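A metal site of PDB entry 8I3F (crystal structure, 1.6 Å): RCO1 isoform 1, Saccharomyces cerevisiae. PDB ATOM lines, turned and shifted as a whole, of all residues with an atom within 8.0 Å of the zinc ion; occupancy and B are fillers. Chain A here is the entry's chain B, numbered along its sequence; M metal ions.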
ATOM      1  N   ASN A   2     -29.893  34.563 -14.034  1.00  0.00           N
ATOM      2  CA  ASN A   2     -29.792  33.591 -12.947  1.00  0.00           C
ATOM      3  C   ASN A   2     -31.155  33.141 -12.462  1.00  0.00           C
ATOM      4  O   ASN A   2     -32.179  33.789 -12.699  1.00  0.00           O
ATOM      5  CB  ASN A   2     -29.000  34.173 -11.771  1.00  0.00           C
ATOM      6  CG  ASN A   2     -27.516  34.270 -12.081  1.00  0.00           C
ATOM      7  OD1 ASN A   2     -27.049  35.279 -12.622  1.00  0.00           O
ATOM      8  ND2 ASN A   2     -26.754  33.241 -11.722  1.00  0.00           N
ATOM      9  N   CYS A  17     -25.645  35.241  -6.823  1.00  0.00           N
ATOM     10  CA  CYS A  17     -25.724  34.634  -8.150  1.00  0.00           C
ATOM     11  C   CYS A  17     -24.352  34.252  -8.663  1.00  0.00           C
ATOM     12  O   CYS A  17     -23.415  35.044  -8.582  1.00  0.00           O
ATOM     13  CB  CYS A  17     -26.384  35.573  -9.160  1.00  0.00           C
ATOM     14  SG  CYS A  17     -28.019  36.065  -8.607  1.00  0.00           S
ATOM     15  N   CYS A  18     -24.271  33.078  -9.276  1.00  0.00           N
ATOM     16  CA  CYS A  18     -23.042  32.659  -9.936  1.00  0.00           C
ATOM     17  C   CYS A  18     -22.804  33.473 -11.192  1.00  0.00           C
ATOM     18  O   CYS A  18     -23.730  33.731 -11.964  1.00  0.00           O
ATOM     19  CB  CYS A  18     -23.100  31.181 -10.325  1.00  0.00           C
ATOM     20  SG  CYS A  18     -21.506  30.600 -10.912  1.00  0.00           S
ATOM     21  N   ASP A  19     -21.551  33.829 -11.428  1.00  0.00           N
ATOM     22  CA  ASP A  19     -21.207  34.613 -12.605  1.00  0.00           C
ATOM     23  C   ASP A  19     -20.861  33.770 -13.826  1.00  0.00           C
ATOM     24  O   ASP A  19     -20.669  34.342 -14.908  1.00  0.00           O
ATOM     25  CB  ASP A  19     -20.050  35.575 -12.285  1.00  0.00           C
ATOM     26  CG  ASP A  19     -20.523  36.807 -11.520  1.00  0.00           C
ATOM     27  OD1 ASP A  19     -21.540  37.385 -11.934  1.00  0.00           O
ATOM     28  OD2 ASP A  19     -19.908  37.176 -10.501  1.00  0.00           O
ATOM     29  N   THR A  20     -20.744  32.454 -13.701  1.00  0.00           N
ATOM     30  CA  THR A  20     -20.445  31.635 -14.869  1.00  0.00           C
ATOM     31  C   THR A  20     -21.504  30.569 -15.116  1.00  0.00           C
ATOM     32  O   THR A  20     -21.353  29.779 -16.057  1.00  0.00           O
ATOM     33  CB  THR A  20     -19.050  31.014 -14.728  1.00  0.00           C
ATOM     34  OG1 THR A  20     -18.815  30.659 -13.363  1.00  0.00           O
ATOM     35  CG2 THR A  20     -17.990  32.006 -15.124  1.00  0.00           C
ATOM     36  N   CYS A  21     -22.591  30.564 -14.355  1.00  0.00           N
ATOM     37  CA  CYS A  21     -23.703  29.637 -14.555  1.00  0.00           C
ATOM     38  C   CYS A  21     -24.955  30.263 -13.950  1.00  0.00           C
ATOM     39  O   CYS A  21     -24.869  31.283 -13.244  1.00  0.00           O
ATOM     40  CB  CYS A  21     -23.371  28.245 -13.956  1.00  0.00           C
ATOM     41  SG  CYS A  21     -23.569  27.984 -12.143  1.00  0.00           S
ATOM     42  N   PRO A  22     -26.146  29.716 -14.234  1.00  0.00           N
ATOM     43  CA  PRO A  22     -27.380  30.395 -13.817  1.00  0.00           C
ATOM     44  C   PRO A  22     -27.749  30.206 -12.348  1.00  0.00           C
ATOM     45  O   PRO A  22     -28.767  30.739 -11.908  1.00  0.00           O
ATOM     46  CB  PRO A  22     -28.446  29.755 -14.715  1.00  0.00           C
ATOM     47  CG  PRO A  22     -27.677  28.995 -15.786  1.00  0.00           C
ATOM     48  CD  PRO A  22     -26.472  28.534 -15.048  1.00  0.00           C
ATOM     49  N   LYS A  23     -26.961  29.458 -11.582  1.00  0.00           N
ATOM     50  CA  LYS A  23     -27.416  29.091 -10.249  1.00  0.00           C
ATOM     51  C   LYS A  23     -27.370  30.271  -9.290  1.00  0.00           C
ATOM     52  O   LYS A  23     -26.528  31.171  -9.398  1.00  0.00           O
ATOM     53  CB  LYS A  23     -26.559  27.944  -9.719  1.00  0.00           C
ATOM     54  CG  LYS A  23     -26.908  26.620 -10.378  1.00  0.00           C
ATOM     55  CD  LYS A  23     -25.787  25.607 -10.235  1.00  0.00           C
ATOM     56  CE  LYS A  23     -26.242  24.248 -10.733  1.00  0.00           C
ATOM     57  NZ  LYS A  23     -27.667  24.000 -10.384  1.00  0.00           N
ATOM     58  N   SER A  24     -28.287  30.256  -8.333  1.00  0.00           N
ATOM     59  CA  SER A  24     -28.345  31.249  -7.268  1.00  0.00           C
ATOM     60  C   SER A  24     -28.460  30.513  -5.956  1.00  0.00           C
ATOM     61  O   SER A  24     -28.997  29.415  -5.905  1.00  0.00           O
ATOM     62  CB  SER A  24     -29.517  32.172  -7.388  1.00  0.00           C
ATOM     63  OG  SER A  24     -29.554  32.758  -8.662  1.00  0.00           O
ATOM     64  N   PHE A  25     -27.974  31.153  -4.897  1.00  0.00           N
ATOM     65  CA  PHE A  25     -27.908  30.491  -3.581  1.00  0.00           C
ATOM     66  C   PHE A  25     -28.225  31.469  -2.465  1.00  0.00           C
ATOM     67  O   PHE A  25     -27.742  32.604  -2.504  1.00  0.00           O
ATOM     68  CB  PHE A  25     -26.511  29.936  -3.328  1.00  0.00           C
ATOM     69  CG  PHE A  25     -26.145  28.763  -4.164  1.00  0.00           C
ATOM     70  CD1 PHE A  25     -25.554  28.923  -5.412  1.00  0.00           C
ATOM     71  CD2 PHE A  25     -26.334  27.468  -3.659  1.00  0.00           C
ATOM     72  CE1 PHE A  25     -25.221  27.797  -6.174  1.00  0.00           C
ATOM     73  CE2 PHE A  25     -26.015  26.360  -4.397  1.00  0.00           C
ATOM     74  CZ  PHE A  25     -25.437  26.503  -5.636  1.00  0.00           C
ATOM     75  N   TRP A  44     -18.151  36.297  -8.540  1.00  0.00           N
ATOM     76  CA  TRP A  44     -18.299  35.169  -7.633  1.00  0.00           C
ATOM     77  C   TRP A  44     -18.756  33.944  -8.409  1.00  0.00           C
ATOM     78  O   TRP A  44     -19.631  34.048  -9.276  1.00  0.00           O
ATOM     79  CB  TRP A  44     -19.270  35.489  -6.472  1.00  0.00           C
ATOM     80  CG  TRP A  44     -19.435  34.291  -5.551  1.00  0.00           C
ATOM     81  CD1 TRP A  44     -18.617  33.924  -4.510  1.00  0.00           C
ATOM     82  CD2 TRP A  44     -20.451  33.287  -5.624  1.00  0.00           C
ATOM     83  NE1 TRP A  44     -19.073  32.747  -3.924  1.00  0.00           N
ATOM     84  CE2 TRP A  44     -20.195  32.345  -4.601  1.00  0.00           C
ATOM     85  CE3 TRP A  44     -21.553  33.076  -6.460  1.00  0.00           C
ATOM     86  CZ2 TRP A  44     -21.008  31.220  -4.404  1.00  0.00           C
ATOM     87  CZ3 TRP A  44     -22.347  31.982  -6.256  1.00  0.00           C
ATOM     88  CH2 TRP A  44     -22.070  31.057  -5.252  1.00  0.00           C
ATOM     89  N   HIS A  45     -18.188  32.783  -8.092  1.00  0.00           N
ATOM     90  CA  HIS A  45     -18.536  31.551  -8.778  1.00  0.00           C
ATOM     91  C   HIS A  45     -18.945  30.463  -7.793  1.00  0.00           C
ATOM     92  O   HIS A  45     -18.345  30.317  -6.713  1.00  0.00           O
ATOM     93  CB  HIS A  45     -17.384  31.047  -9.612  1.00  0.00           C
ATOM     94  CG  HIS A  45     -16.780  32.109 -10.481  1.00  0.00           C
ATOM     95  ND1 HIS A  45     -17.272  32.407 -11.728  1.00  0.00           N
ATOM     96  CD2 HIS A  45     -15.780  32.979 -10.246  1.00  0.00           C
ATOM     97  CE1 HIS A  45     -16.569  33.398 -12.257  1.00  0.00           C
ATOM     98  NE2 HIS A  45     -15.656  33.759 -11.376  1.00  0.00           N
ATOM     99  N   CYS A  46     -19.937  29.659  -8.177  1.00  0.00           N
ATOM    100  CA  CYS A  46     -20.351  28.548  -7.317  1.00  0.00           C
ATOM    101  C   CYS A  46     -19.256  27.482  -7.260  1.00  0.00           C
ATOM    102  O   CYS A  46     -18.309  27.492  -8.054  1.00  0.00           O
ATOM    103  CB  CYS A  46     -21.686  27.960  -7.803  1.00  0.00           C
ATOM    104  SG  CYS A  46     -21.696  27.058  -9.422  1.00  0.00           S
ATOM    105  N   ASN A  47     -19.397  26.561  -6.282  1.00  0.00           N
ATOM    106  CA  ASN A  47     -18.374  25.535  -6.092  1.00  0.00           C
ATOM    107  C   ASN A  47     -18.187  24.722  -7.372  1.00  0.00           C
ATOM    108  O   ASN A  47     -17.052  24.423  -7.761  1.00  0.00           O
ATOM    109  CB  ASN A  47     -18.731  24.606  -4.917  1.00  0.00           C
ATOM    110  CG  ASN A  47     -18.628  25.292  -3.552  1.00  0.00           C
ATOM    111  OD1 ASN A  47     -18.390  26.505  -3.465  1.00  0.00           O
ATOM    112  ND2 ASN A  47     -18.809  24.511  -2.470  1.00  0.00           N
ATOM    113  N   GLU A  48     -19.292  24.390  -8.063  1.00  0.00           N
ATOM    114  CA  GLU A  48     -19.230  23.610  -9.300  1.00  0.00           C
ATOM    115  C   GLU A  48     -18.433  24.337 -10.375  1.00  0.00           C
ATOM    116  O   GLU A  48     -17.556  23.740 -11.016  1.00  0.00           O
ATOM    117  CB  GLU A  48     -20.651  23.318  -9.802  1.00  0.00           C
ATOM    118  CG  GLU A  48     -21.081  21.888  -9.590  1.00  0.00           C
ATOM    119  CD  GLU A  48     -22.590  21.694  -9.605  1.00  0.00           C
ATOM    120  OE1 GLU A  48     -23.203  22.036 -10.631  1.00  0.00           O
ATOM    121  OE2 GLU A  48     -23.135  21.158  -8.596  1.00  0.00           O
ATOM    122  N   CYS A  49     -18.731  25.631 -10.578  1.00  0.00           N
ATOM    123  CA  CYS A  49     -17.960  26.443 -11.519  1.00  0.00           C
ATOM    124  C   CYS A  49     -16.518  26.606 -11.081  1.00  0.00           C
ATOM    125  O   CYS A  49     -15.601  26.548 -11.909  1.00  0.00           O
ATOM    126  CB  CYS A  49     -18.612  27.817 -11.648  1.00  0.00           C
ATOM    127  SG  CYS A  49     -20.054  27.743 -12.702  1.00  0.00           S
ATOM    128  N   LYS A  50     -16.297  26.837  -9.783  1.00  0.00           N
ATOM    129  CA  LYS A  50     -14.942  26.961  -9.261  1.00  0.00           C
ATOM    130  C   LYS A  50     -14.117  25.739  -9.614  1.00  0.00           C
ATOM    131  O   LYS A  50     -12.934  25.848  -9.982  1.00  0.00           O
ATOM    132  CB  LYS A  50     -14.991  27.142  -7.747  1.00  0.00           C
ATOM    133  CG  LYS A  50     -14.811  28.564  -7.229  1.00  0.00           C
ATOM    134  CD  LYS A  50     -14.774  28.594  -5.708  1.00  0.00           C
ATOM    135  N   LYS A  52     -14.585  23.551 -12.158  1.00  0.00           N
ATOM    136  CA  LYS A  52     -14.280  23.515 -13.588  1.00  0.00           C
ATOM    137  C   LYS A  52     -13.249  24.573 -13.953  1.00  0.00           C
ATOM    138  O   LYS A  52     -12.382  24.344 -14.805  1.00  0.00           O
ATOM    139  CB  LYS A  52     -15.555  23.709 -14.402  1.00  0.00           C
ATOM    140  CG  LYS A  52     -16.642  22.718 -14.065  1.00  0.00           C
ATOM    141  CD  LYS A  52     -17.997  23.126 -14.623  1.00  0.00           C
ATOM    142  CE  LYS A  52     -18.792  21.900 -15.065  1.00  0.00           C
ATOM    143  NZ  LYS A  52     -20.209  22.236 -15.417  1.00  0.00           N
ATOM    144  N   ILE A  53     -13.321  25.747 -13.305  1.00  0.00           N
ATOM    145  CA  ILE A  53     -12.305  26.774 -13.517  1.00  0.00           C
ATOM    146  C   ILE A  53     -10.939  26.251 -13.078  1.00  0.00           C
ATOM    147  O   ILE A  53      -9.922  26.461 -13.749  1.00  0.00           O
ATOM    148  CB  ILE A  53     -12.673  28.075 -12.783  1.00  0.00           C
ATOM    149  CG1 ILE A  53     -13.823  28.802 -13.502  1.00  0.00           C
ATOM    150  CG2 ILE A  53     -11.437  28.980 -12.656  1.00  0.00           C
ATOM    151  CD1 ILE A  53     -14.509  29.896 -12.675  1.00  0.00           C
ATOM    152  N   ASN A  90     -21.984  21.341  -5.888  1.00  0.00           N
ATOM    153  CA  ASN A  90     -22.447  22.451  -5.068  1.00  0.00           C
ATOM    154  C   ASN A  90     -23.074  21.959  -3.768  1.00  0.00           C
ATOM    155  O   ASN A  90     -23.563  20.830  -3.688  1.00  0.00           O
ATOM    156  CB  ASN A  90     -23.498  23.238  -5.824  1.00  0.00           C
ATOM    157  CG  ASN A  90     -22.875  24.189  -6.814  1.00  0.00           C
ATOM    158  OD1 ASN A  90     -21.743  24.612  -6.626  1.00  0.00           O
ATOM    159  ND2 ASN A  90     -23.626  24.512  -7.872  1.00  0.00           N
HETATM  160 ZN    ZN M   1     -21.805  28.314 -11.243  1.00  0.00          ZN
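The zinc ion is bound by SG of Cys 21, SG of Cys 46, SG of Cys 18 and SG of Cys 49.
The zinc ion has four donor atoms within binding distance.
Of the 20 residues printed, 4 come within 4 Å of the zinc ion.
The side-chain sulfur (SG) of Cys 21 lies close to the backbone NH (N) of Lys 23.
The backbone carbonyl oxygen (O) of Cys 21 sits at hydrogen-bond distance from the side-chain amide nitrogen (ND2) of Asn 2 (3.1 Å).
The side-chain amide nitrogen (ND2) of Asn 90 sits close to the side-chain sulfur (SG) of Cys 46.
The side-chain sulfur (SG) of Cys 18 sits close to the backbone NH (N) of Thr 20 (3.4 Å).
The backbone carbonyl oxygen (O) of Lys 23 is in hydrogen-bond range of the backbone NH (N) of Cys 18 (3.0 Å).
O of Cys 18 sits at hydrogen-bond distance from ND2 of Asn 2, 3.1 Å away.
SG of Cys 49 lies close to OG1 of Thr 20 (3.2 Å).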
